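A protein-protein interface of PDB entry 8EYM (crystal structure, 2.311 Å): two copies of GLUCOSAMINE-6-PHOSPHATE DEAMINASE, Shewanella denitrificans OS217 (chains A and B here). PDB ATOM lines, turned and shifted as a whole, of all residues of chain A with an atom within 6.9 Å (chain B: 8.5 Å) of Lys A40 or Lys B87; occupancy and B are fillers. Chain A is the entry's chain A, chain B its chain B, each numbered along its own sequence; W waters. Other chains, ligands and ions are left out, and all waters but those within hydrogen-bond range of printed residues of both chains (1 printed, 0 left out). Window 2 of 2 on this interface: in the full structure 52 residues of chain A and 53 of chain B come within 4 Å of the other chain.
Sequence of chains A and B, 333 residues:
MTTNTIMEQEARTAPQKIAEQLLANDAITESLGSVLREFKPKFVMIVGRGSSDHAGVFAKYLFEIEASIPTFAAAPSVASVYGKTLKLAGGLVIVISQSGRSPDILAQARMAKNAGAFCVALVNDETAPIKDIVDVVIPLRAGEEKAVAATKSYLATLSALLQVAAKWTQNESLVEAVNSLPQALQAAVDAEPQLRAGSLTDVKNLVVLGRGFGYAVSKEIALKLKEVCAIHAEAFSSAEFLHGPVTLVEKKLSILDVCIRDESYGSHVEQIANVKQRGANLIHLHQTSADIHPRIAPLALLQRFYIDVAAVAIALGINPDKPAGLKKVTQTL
O of Pro A41 is in hydrogen-bond range of NZ of Lys B87.
O of Thr B85 is in hydrogen-bond range of OG of Ser A68, at 3.4 Å.
The backbone carbonyl oxygen of Ser A68 lies within hydrogen-bond range of the backbone NH of Lys B87 (2.8 Å).
O of Lys A40 is in hydrogen-bond range of NZ of Lys A42 (3.1 Å).
Among the printed residues, pairs that only touch across the chains: Lys A40 with Lys B87, Ser A68 with Leu B86, Ile A69 with Lys B87, Pro A70 with Phe B72, Pro A70 with Lys B87 and Pro A70 with Leu B88.
Lys A40 touches just one residue of chain B: Lys B87 (3.8 Å).
Pro A41 touches just one residue of chain B: Lys B87 (2.8 Å).
Of the printed residues of chain B, Ile A69 touches Lys B87.
Of the printed residues of chain A, Phe B72 touches Pro A70 (3.8 Å).
Of chain A, only Lys A40 (3.8 Å), Pro A41 (2.8 Å), Ser A68 (2.8 Å), Ile A69 (3.5 Å) and Pro A70 (3.3 Å) come within 4 Å of Lys B87.
Printed residues of chain A within 4 Å of Leu B88: Pro A70 (3.6 Å).
The nearest residue of chain B that does not touch Lys A40 is Lys B42 (8.2 Å).
The nearest residue of chain A that does not touch Lys B87 is Lys A42 (4.3 Å).
The nearest printed residue of chain A that does not touch Phe B72 is Phe A43 (5.6 Å).
Of the 18 printed residues of chain B, 5 touch a printed residue of chain A.
Printed residues of chain B that touch a printed residue of chain A: Phe B72, Thr B85, Leu B86, Lys B87 and Leu B88.
Hydrophobic or aromatic side chains of chain A that line the printed part of chain B: Ile A69 and Pro A70.
Among the printed residues, 9 pairs touch across the chains.
4 positions are printed for both chains.
Of the 9 pairs that touch across the chains among the printed residues, none has its exchanged pair printed and touching as well.
Water W1 bridges O of Lys A42 and O of Lys B87.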
ATOM      1  N   SER A  34     -10.153 -15.469 -24.235  1.00  0.00           N
ATOM      2  CA  SER A  34     -11.312 -16.353 -24.236  1.00  0.00           C
ATOM      3  C   SER A  34     -11.372 -17.187 -22.962  1.00  0.00           C
ATOM      4  O   SER A  34     -12.461 -17.422 -22.424  1.00  0.00           O
ATOM      5  CB  SER A  34     -11.308 -17.240 -25.483  1.00  0.00           C
ATOM      6  OG  SER A  34     -10.390 -18.314 -25.351  1.00  0.00           O
ATOM      7  N   VAL A  35     -10.214 -17.647 -22.470  1.00  0.00           N
ATOM      8  CA  VAL A  35     -10.168 -18.349 -21.190  1.00  0.00           C
ATOM      9  C   VAL A  35     -10.717 -17.463 -20.078  1.00  0.00           C
ATOM     10  O   VAL A  35     -11.491 -17.914 -19.226  1.00  0.00           O
ATOM     11  CB  VAL A  35      -8.735 -18.814 -20.879  1.00  0.00           C
ATOM     12  CG1 VAL A  35      -8.684 -19.439 -19.481  1.00  0.00           C
ATOM     13  CG2 VAL A  35      -8.244 -19.793 -21.936  1.00  0.00           C
ATOM     14  N   LEU A  36     -10.309 -16.190 -20.061  1.00  0.00           N
ATOM     15  CA  LEU A  36     -10.778 -15.263 -19.035  1.00  0.00           C
ATOM     16  C   LEU A  36     -12.255 -14.949 -19.213  1.00  0.00           C
ATOM     17  O   LEU A  36     -12.973 -14.763 -18.221  1.00  0.00           O
ATOM     18  CB  LEU A  36      -9.953 -13.973 -19.075  1.00  0.00           C
ATOM     19  CG  LEU A  36      -8.479 -14.076 -18.667  1.00  0.00           C
ATOM     20  CD1 LEU A  36      -7.753 -12.751 -18.904  1.00  0.00           C
ATOM     21  CD2 LEU A  36      -8.365 -14.513 -17.223  1.00  0.00           C
ATOM     22  N   ARG A  37     -12.731 -14.900 -20.463  1.00  0.00           N
ATOM     23  CA  ARG A  37     -14.156 -14.661 -20.692  1.00  0.00           C
ATOM     24  C   ARG A  37     -14.987 -15.827 -20.192  1.00  0.00           C
ATOM     25  O   ARG A  37     -16.129 -15.628 -19.766  1.00  0.00           O
ATOM     26  CB  ARG A  37     -14.455 -14.376 -22.169  1.00  0.00           C
ATOM     27  CG  ARG A  37     -14.419 -12.898 -22.560  1.00  0.00           C
ATOM     28  CD  ARG A  37     -15.002 -12.641 -23.959  1.00  0.00           C
ATOM     29  NE  ARG A  37     -14.444 -13.542 -24.966  1.00  0.00           N
ATOM     30  CZ  ARG A  37     -13.240 -13.407 -25.517  1.00  0.00           C
ATOM     31  NH1 ARG A  37     -12.480 -12.359 -25.230  1.00  0.00           N
ATOM     32  NH2 ARG A  37     -12.822 -14.290 -26.408  1.00  0.00           N
ATOM     33  N   GLU A  38     -14.429 -17.041 -20.221  1.00  0.00           N
ATOM     34  CA  GLU A  38     -15.110 -18.199 -19.647  1.00  0.00           C
ATOM     35  C   GLU A  38     -14.904 -18.267 -18.135  1.00  0.00           C
ATOM     36  O   GLU A  38     -15.863 -18.465 -17.384  1.00  0.00           O
ATOM     37  CB  GLU A  38     -14.651 -19.493 -20.339  1.00  0.00           C
ATOM     38  N   PHE A  39     -13.661 -18.076 -17.675  1.00  0.00           N
ATOM     39  CA  PHE A  39     -13.341 -18.171 -16.249  1.00  0.00           C
ATOM     40  C   PHE A  39     -14.090 -17.123 -15.425  1.00  0.00           C
ATOM     41  O   PHE A  39     -14.535 -17.405 -14.306  1.00  0.00           O
ATOM     42  CB  PHE A  39     -11.830 -18.011 -16.063  1.00  0.00           C
ATOM     43  CG  PHE A  39     -11.358 -18.164 -14.639  1.00  0.00           C
ATOM     44  CD1 PHE A  39     -11.423 -19.389 -13.995  1.00  0.00           C
ATOM     45  CD2 PHE A  39     -10.802 -17.088 -13.958  1.00  0.00           C
ATOM     46  CE1 PHE A  39     -10.969 -19.533 -12.689  1.00  0.00           C
ATOM     47  CE2 PHE A  39     -10.349 -17.231 -12.645  1.00  0.00           C
ATOM     48  CZ  PHE A  39     -10.436 -18.450 -12.016  1.00  0.00           C
ATOM     49  N   LYS A  40     -14.238 -15.905 -15.962  1.00  0.00           N
ATOM     50  CA  LYS A  40     -14.891 -14.778 -15.296  1.00  0.00           C
ATOM     51  C   LYS A  40     -14.292 -14.532 -13.910  1.00  0.00           C
ATOM     52  O   LYS A  40     -14.965 -14.757 -12.892  1.00  0.00           O
ATOM     53  CB  LYS A  40     -16.404 -15.027 -15.220  1.00  0.00           C
ATOM     54  N   PRO A  41     -13.044 -14.051 -13.835  1.00  0.00           N
ATOM     55  CA  PRO A  41     -12.371 -13.922 -12.534  1.00  0.00           C
ATOM     56  C   PRO A  41     -13.103 -12.966 -11.608  1.00  0.00           C
ATOM     57  O   PRO A  41     -13.636 -11.942 -12.038  1.00  0.00           O
ATOM     58  CB  PRO A  41     -10.985 -13.386 -12.902  1.00  0.00           C
ATOM     59  CG  PRO A  41     -11.150 -12.777 -14.235  1.00  0.00           C
ATOM     60  CD  PRO A  41     -12.189 -13.593 -14.942  1.00  0.00           C
ATOM     61  N   LYS A  42     -13.151 -13.331 -10.326  1.00  0.00           N
ATOM     62  CA  LYS A  42     -13.783 -12.468  -9.337  1.00  0.00           C
ATOM     63  C   LYS A  42     -12.920 -11.268  -8.994  1.00  0.00           C
ATOM     64  O   LYS A  42     -13.451 -10.242  -8.568  1.00  0.00           O
ATOM     65  CB  LYS A  42     -14.114 -13.272  -8.086  1.00  0.00           C
ATOM     66  CG  LYS A  42     -15.054 -14.455  -8.350  1.00  0.00           C
ATOM     67  CD  LYS A  42     -16.411 -14.038  -8.938  1.00  0.00           C
ATOM     68  CE  LYS A  42     -17.242 -15.267  -9.341  1.00  0.00           C
ATOM     69  NZ  LYS A  42     -16.725 -15.946 -10.576  1.00  0.00           N
ATOM     70  N   PHE A  43     -11.611 -11.369  -9.196  1.00  0.00           N
ATOM     71  CA  PHE A  43     -10.666 -10.308  -8.886  1.00  0.00           C
ATOM     72  C   PHE A  43      -9.352 -10.668  -9.567  1.00  0.00           C
ATOM     73  O   PHE A  43      -9.134 -11.817  -9.968  1.00  0.00           O
ATOM     74  CB  PHE A  43     -10.464 -10.138  -7.374  1.00  0.00           C
ATOM     75  CG  PHE A  43      -9.957 -11.374  -6.684  1.00  0.00           C
ATOM     76  CD1 PHE A  43      -8.615 -11.725  -6.745  1.00  0.00           C
ATOM     77  CD2 PHE A  43     -10.824 -12.187  -5.974  1.00  0.00           C
ATOM     78  CE1 PHE A  43      -8.153 -12.856  -6.113  1.00  0.00           C
ATOM     79  CE2 PHE A  43     -10.357 -13.316  -5.343  1.00  0.00           C
ATOM     80  CZ  PHE A  43      -9.017 -13.651  -5.415  1.00  0.00           C
ATOM     81  N   ALA A  67     -12.452  -3.633 -17.583  1.00  0.00           N
ATOM     82  CA  ALA A  67     -13.082  -4.931 -17.423  1.00  0.00           C
ATOM     83  C   ALA A  67     -13.968  -5.035 -16.183  1.00  0.00           C
ATOM     84  O   ALA A  67     -14.567  -6.089 -15.965  1.00  0.00           O
ATOM     85  CB  ALA A  67     -11.997  -6.011 -17.382  1.00  0.00           C
ATOM     86  N   SER A  68     -14.056  -3.986 -15.358  1.00  0.00           N
ATOM     87  CA  SER A  68     -14.887  -3.952 -14.150  1.00  0.00           C
ATOM     88  C   SER A  68     -14.486  -4.997 -13.108  1.00  0.00           C
ATOM     89  O   SER A  68     -15.315  -5.382 -12.277  1.00  0.00           O
ATOM     90  CB  SER A  68     -16.377  -4.097 -14.472  1.00  0.00           C
ATOM     91  OG  SER A  68     -16.811  -3.035 -15.288  1.00  0.00           O
ATOM     92  N   ILE A  69     -13.248  -5.477 -13.124  1.00  0.00           N
ATOM     93  CA  ILE A  69     -12.801  -6.523 -12.211  1.00  0.00           C
ATOM     94  C   ILE A  69     -11.936  -5.864 -11.137  1.00  0.00           C
ATOM     95  O   ILE A  69     -10.934  -5.223 -11.487  1.00  0.00           O
ATOM     96  CB  ILE A  69     -12.015  -7.624 -12.941  1.00  0.00           C
ATOM     97  CG1 ILE A  69     -12.871  -8.225 -14.077  1.00  0.00           C
ATOM     98  CG2 ILE A  69     -11.561  -8.687 -11.954  1.00  0.00           C
ATOM     99  CD1 ILE A  69     -14.284  -8.619 -13.635  1.00  0.00           C
ATOM    100  N   PRO A  70     -12.301  -5.980  -9.855  1.00  0.00           N
ATOM    101  CA  PRO A  70     -11.453  -5.461  -8.770  1.00  0.00           C
ATOM    102  C   PRO A  70     -10.043  -6.038  -8.840  1.00  0.00           C
ATOM    103  O   PRO A  70      -9.860  -7.249  -8.956  1.00  0.00           O
ATOM    104  CB  PRO A  70     -12.184  -5.936  -7.506  1.00  0.00           C
ATOM    105  CG  PRO A  70     -13.574  -6.221  -7.932  1.00  0.00           C
ATOM    106  CD  PRO A  70     -13.520  -6.639  -9.350  1.00  0.00           C
ATOM    107  N   GLY A  90     -11.230 -18.857  -7.822  1.00  0.00           N
ATOM    108  CA  GLY A  90     -12.056 -18.010  -8.656  1.00  0.00           C
ATOM    109  C   GLY A  90     -11.428 -16.687  -9.032  1.00  0.00           C
ATOM    110  O   GLY A  90     -12.094 -15.870  -9.679  1.00  0.00           O
ATOM    111  N   GLY A  91     -10.181 -16.447  -8.629  1.00  0.00           N
ATOM    112  CA  GLY A  91      -9.470 -15.236  -8.967  1.00  0.00           C
ATOM    113  C   GLY A  91      -8.299 -15.431  -9.909  1.00  0.00           C
ATOM    114  O   GLY A  91      -7.744 -16.533 -10.038  1.00  0.00           O
ATOM    115  N   TRP A 168      -9.353  -9.641 -23.946  1.00  0.00           N
ATOM    116  CA  TRP A 168     -10.336 -10.124 -22.979  1.00  0.00           C
ATOM    117  C   TRP A 168     -11.649  -9.350 -23.082  1.00  0.00           C
ATOM    118  O   TRP A 168     -12.723  -9.941 -23.247  1.00  0.00           O
ATOM    119  CB  TRP A 168      -9.716 -10.034 -21.580  1.00  0.00           C
ATOM    120  CG  TRP A 168     -10.603 -10.290 -20.386  1.00  0.00           C
ATOM    121  CD1 TRP A 168     -11.844 -10.859 -20.372  1.00  0.00           C
ATOM    122  CD2 TRP A 168     -10.289  -9.982 -19.027  1.00  0.00           C
ATOM    123  NE1 TRP A 168     -12.325 -10.920 -19.089  1.00  0.00           N
ATOM    124  CE2 TRP A 168     -11.389 -10.393 -18.239  1.00  0.00           C
ATOM    125  CE3 TRP A 168      -9.180  -9.395 -18.393  1.00  0.00           C
ATOM    126  CZ2 TRP A 168     -11.419 -10.235 -16.850  1.00  0.00           C
ATOM    127  CZ3 TRP A 168      -9.207  -9.240 -17.005  1.00  0.00           C
ATOM    128  CH2 TRP A 168     -10.326  -9.657 -16.251  1.00  0.00           C
ATOM    129  N   LYS B  42     -15.662 -12.920  -0.569  1.00  0.00           N
ATOM    130  CA  LYS B  42     -14.610 -13.263  -1.513  1.00  0.00           C
ATOM    131  C   LYS B  42     -13.404 -12.352  -1.352  1.00  0.00           C
ATOM    132  O   LYS B  42     -12.288 -12.759  -1.694  1.00  0.00           O
ATOM    133  CB  LYS B  42     -15.131 -13.110  -2.943  1.00  0.00           C
ATOM    134  CG  LYS B  42     -16.307 -14.031  -3.284  1.00  0.00           C
ATOM    135  CD  LYS B  42     -16.934 -13.714  -4.649  1.00  0.00           C
ATOM    136  CE  LYS B  42     -17.713 -14.920  -5.183  1.00  0.00           C
ATOM    137  NZ  LYS B  42     -18.402 -15.672  -4.083  1.00  0.00           N
ATOM    138  N   PHE B  43     -13.608 -11.141  -0.830  1.00  0.00           N
ATOM    139  CA  PHE B  43     -12.545 -10.162  -0.681  1.00  0.00           C
ATOM    140  C   PHE B  43     -13.060  -9.016   0.182  1.00  0.00           C
ATOM    141  O   PHE B  43     -14.271  -8.846   0.360  1.00  0.00           O
ATOM    142  CB  PHE B  43     -12.055  -9.655  -2.046  1.00  0.00           C
ATOM    143  CG  PHE B  43     -13.135  -9.004  -2.889  1.00  0.00           C
ATOM    144  CD1 PHE B  43     -13.568  -7.705  -2.624  1.00  0.00           C
ATOM    145  CD2 PHE B  43     -13.682  -9.670  -3.966  1.00  0.00           C
ATOM    146  CE1 PHE B  43     -14.563  -7.107  -3.401  1.00  0.00           C
ATOM    147  CE2 PHE B  43     -14.662  -9.074  -4.751  1.00  0.00           C
ATOM    148  CZ  PHE B  43     -15.102  -7.804  -4.474  1.00  0.00           C
ATOM    149  N   MET B  45     -12.643  -4.890   0.260  1.00  0.00           N
ATOM    150  CA  MET B  45     -12.186  -3.651  -0.359  1.00  0.00           C
ATOM    151  C   MET B  45     -12.378  -2.503   0.625  1.00  0.00           C
ATOM    152  O   MET B  45     -13.459  -2.343   1.198  1.00  0.00           O
ATOM    153  CB  MET B  45     -12.947  -3.371  -1.661  1.00  0.00           C
ATOM    154  CG  MET B  45     -12.484  -2.121  -2.379  1.00  0.00           C
ATOM    155  SD  MET B  45     -13.289  -1.903  -3.983  1.00  0.00           S
ATOM    156  CE  MET B  45     -14.821  -1.118  -3.492  1.00  0.00           C
ATOM    157  N   PHE B  72      -7.740  -5.155   0.039  1.00  0.00           N
ATOM    158  CA  PHE B  72      -7.052  -4.148  -0.758  1.00  0.00           C
ATOM    159  C   PHE B  72      -7.837  -2.847  -0.710  1.00  0.00           C
ATOM    160  O   PHE B  72      -8.994  -2.812  -0.290  1.00  0.00           O
ATOM    161  CB  PHE B  72      -6.920  -4.624  -2.198  1.00  0.00           C
ATOM    162  CG  PHE B  72      -8.247  -4.869  -2.865  1.00  0.00           C
ATOM    163  CD1 PHE B  72      -8.885  -6.095  -2.737  1.00  0.00           C
ATOM    164  CD2 PHE B  72      -8.880  -3.857  -3.582  1.00  0.00           C
ATOM    165  CE1 PHE B  72     -10.112  -6.322  -3.329  1.00  0.00           C
ATOM    166  CE2 PHE B  72     -10.105  -4.081  -4.171  1.00  0.00           C
ATOM    167  CZ  PHE B  72     -10.723  -5.315  -4.041  1.00  0.00           C
ATOM    168  N   LYS B  84     -17.053   4.320 -13.370  1.00  0.00           N
ATOM    169  CA  LYS B  84     -17.275   2.894 -13.557  1.00  0.00           C
ATOM    170  C   LYS B  84     -17.759   2.269 -12.268  1.00  0.00           C
ATOM    171  O   LYS B  84     -17.460   2.745 -11.170  1.00  0.00           O
ATOM    172  CB  LYS B  84     -16.008   2.164 -14.000  1.00  0.00           C
ATOM    173  CG  LYS B  84     -15.365   2.760 -15.216  1.00  0.00           C
ATOM    174  CD  LYS B  84     -16.289   2.670 -16.416  1.00  0.00           C
ATOM    175  CE  LYS B  84     -15.615   3.248 -17.649  1.00  0.00           C
ATOM    176  NZ  LYS B  84     -16.366   2.939 -18.897  1.00  0.00           N
ATOM    177  N   THR B  85     -18.547   1.216 -12.420  1.00  0.00           N
ATOM    178  CA  THR B  85     -18.960   0.359 -11.328  1.00  0.00           C
ATOM    179  C   THR B  85     -18.152  -0.922 -11.450  1.00  0.00           C
ATOM    180  O   THR B  85     -17.803  -1.347 -12.553  1.00  0.00           O
ATOM    181  CB  THR B  85     -20.460   0.088 -11.452  1.00  0.00           C
ATOM    182  OG1 THR B  85     -21.135   1.343 -11.652  1.00  0.00           O
ATOM    183  CG2 THR B  85     -21.010  -0.590 -10.205  1.00  0.00           C
ATOM    184  N   LEU B  86     -17.837  -1.540 -10.328  1.00  0.00           N
ATOM    185  CA  LEU B  86     -17.061  -2.765 -10.379  1.00  0.00           C
ATOM    186  C   LEU B  86     -17.966  -3.946 -10.091  1.00  0.00           C
ATOM    187  O   LEU B  86     -19.062  -3.791  -9.549  1.00  0.00           O
ATOM    188  CB  LEU B  86     -15.905  -2.736  -9.387  1.00  0.00           C
ATOM    189  CG  LEU B  86     -14.827  -1.686  -9.610  1.00  0.00           C
ATOM    190  CD1 LEU B  86     -13.889  -1.597  -8.399  1.00  0.00           C
ATOM    191  CD2 LEU B  86     -14.067  -1.964 -10.891  1.00  0.00           C
ATOM    192  N   LYS B  87     -17.527  -5.123 -10.515  1.00  0.00           N
ATOM    193  CA  LYS B  87     -18.192  -6.360 -10.109  1.00  0.00           C
ATOM    194  C   LYS B  87     -17.779  -6.666  -8.668  1.00  0.00           C
ATOM    195  O   LYS B  87     -16.672  -7.150  -8.416  1.00  0.00           O
ATOM    196  CB  LYS B  87     -17.820  -7.491 -11.067  1.00  0.00           C
ATOM    197  CG  LYS B  87     -18.749  -8.700 -11.031  1.00  0.00           C
ATOM    198  CD  LYS B  87     -18.247  -9.773 -11.993  1.00  0.00           C
ATOM    199  CE  LYS B  87     -16.926 -10.366 -11.519  1.00  0.00           C
ATOM    200  NZ  LYS B  87     -16.317 -11.221 -12.561  1.00  0.00           N
ATOM    201  N   LEU B  88     -18.657  -6.362  -7.707  1.00  0.00           N
ATOM    202  CA  LEU B  88     -18.366  -6.598  -6.293  1.00  0.00           C
ATOM    203  C   LEU B  88     -19.306  -7.574  -5.603  1.00  0.00           C
ATOM    204  O   LEU B  88     -19.195  -7.741  -4.385  1.00  0.00           O
ATOM    205  CB  LEU B  88     -18.356  -5.287  -5.488  1.00  0.00           C
ATOM    206  CG  LEU B  88     -17.407  -4.175  -5.926  1.00  0.00           C
ATOM    207  CD1 LEU B  88     -17.753  -2.891  -5.200  1.00  0.00           C
ATOM    208  CD2 LEU B  88     -15.969  -4.580  -5.720  1.00  0.00           C
ATOM    209  N   ALA B  89     -20.240  -8.195  -6.322  1.00  0.00           N
ATOM    210  CA  ALA B  89     -21.170  -9.130  -5.703  1.00  0.00           C
ATOM    211  C   ALA B  89     -20.412 -10.176  -4.902  1.00  0.00           C
ATOM    212  O   ALA B  89     -19.434 -10.752  -5.378  1.00  0.00           O
ATOM    213  CB  ALA B  89     -21.980  -9.826  -6.797  1.00  0.00           C
ATOM    214  N   GLY B  90     -20.859 -10.406  -3.668  1.00  0.00           N
ATOM    215  CA  GLY B  90     -20.205 -11.373  -2.818  1.00  0.00           C
ATOM    216  C   GLY B  90     -18.963 -10.883  -2.113  1.00  0.00           C
ATOM    217  O   GLY B  90     -18.330 -11.666  -1.394  1.00  0.00           O
ATOM    218  N   GLY B  91     -18.602  -9.615  -2.273  1.00  0.00           N
ATOM    219  CA  GLY B  91     -17.467  -9.057  -1.562  1.00  0.00           C
ATOM    220  C   GLY B  91     -17.896  -8.109  -0.461  1.00  0.00           C
ATOM    221  O   GLY B  91     -19.029  -7.614  -0.462  1.00  0.00           O
ATOM    222  N   VAL B  93     -17.243  -4.531   1.495  1.00  0.00           N
ATOM    223  CA  VAL B  93     -16.658  -3.204   1.344  1.00  0.00           C
ATOM    224  C   VAL B  93     -16.742  -2.477   2.675  1.00  0.00           C
ATOM    225  O   VAL B  93     -17.831  -2.324   3.236  1.00  0.00           O
ATOM    226  CB  VAL B  93     -17.361  -2.408   0.234  1.00  0.00           C
ATOM    227  CG1 VAL B  93     -17.045  -0.924   0.345  1.00  0.00           C
ATOM    228  CG2 VAL B  93     -16.927  -2.943  -1.129  1.00  0.00           C
ATOM    229  N   MET B 111     -21.346   3.622  -5.362  1.00  0.00           N
ATOM    230  CA  MET B 111     -21.122   2.636  -6.436  1.00  0.00           C
ATOM    231  C   MET B 111     -20.889   1.255  -5.838  1.00  0.00           C
ATOM    232  O   MET B 111     -21.476   0.329  -6.312  1.00  0.00           O
ATOM    233  CB  MET B 111     -19.911   3.040  -7.260  1.00  0.00           C
ATOM    234  CG  MET B 111     -19.817   4.504  -7.480  1.00  0.00           C
ATOM    235  SD  MET B 111     -20.934   5.257  -8.663  1.00  0.00           S
ATOM    236  CE  MET B 111     -20.338   4.357 -10.085  1.00  0.00           C
ATOM    237  N   ALA B 112     -20.211   1.114  -4.717  1.00  0.00           N
ATOM    238  CA  ALA B 112     -20.056  -0.219  -4.103  1.00  0.00           C
ATOM    239  C   ALA B 112     -21.428  -0.742  -3.667  1.00  0.00           C
ATOM    240  O   ALA B 112     -21.701  -1.907  -3.835  1.00  0.00           O
ATOM    241  CB  ALA B 112     -19.069  -0.162  -2.970  1.00  0.00           C
ATOM    242  N   ALA B 115     -23.365  -1.940  -6.608  1.00  0.00           N
ATOM    243  CA  ALA B 115     -22.792  -3.129  -7.233  1.00  0.00           C
ATOM    244  C   ALA B 115     -23.119  -4.424  -6.499  1.00  0.00           C
ATOM    245  O   ALA B 115     -22.632  -5.485  -6.901  1.00  0.00           O
ATOM    246  CB  ALA B 115     -21.275  -2.976  -7.358  1.00  0.00           C
ATOM    247  N   GLY B 116     -23.906  -4.380  -5.436  1.00  0.00           N
ATOM    248  CA  GLY B 116     -24.255  -5.604  -4.741  1.00  0.00           C
ATOM    249  C   GLY B 116     -23.275  -6.054  -3.677  1.00  0.00           C
ATOM    250  O   GLY B 116     -23.352  -7.207  -3.237  1.00  0.00           O
ATOM    251  N   ALA B 117     -22.337  -5.198  -3.269  1.00  0.00           N
ATOM    252  CA  ALA B 117     -21.431  -5.555  -2.191  1.00  0.00           C
ATOM    253  C   ALA B 117     -22.098  -5.290  -0.839  1.00  0.00           C
ATOM    254  O   ALA B 117     -22.881  -4.353  -0.679  1.00  0.00           O
ATOM    255  CB  ALA B 117     -20.129  -4.761  -2.316  1.00  0.00           C
HETATM  256  O   HOH W   1     -16.006  -9.854  -8.013  1.00  0.00           O
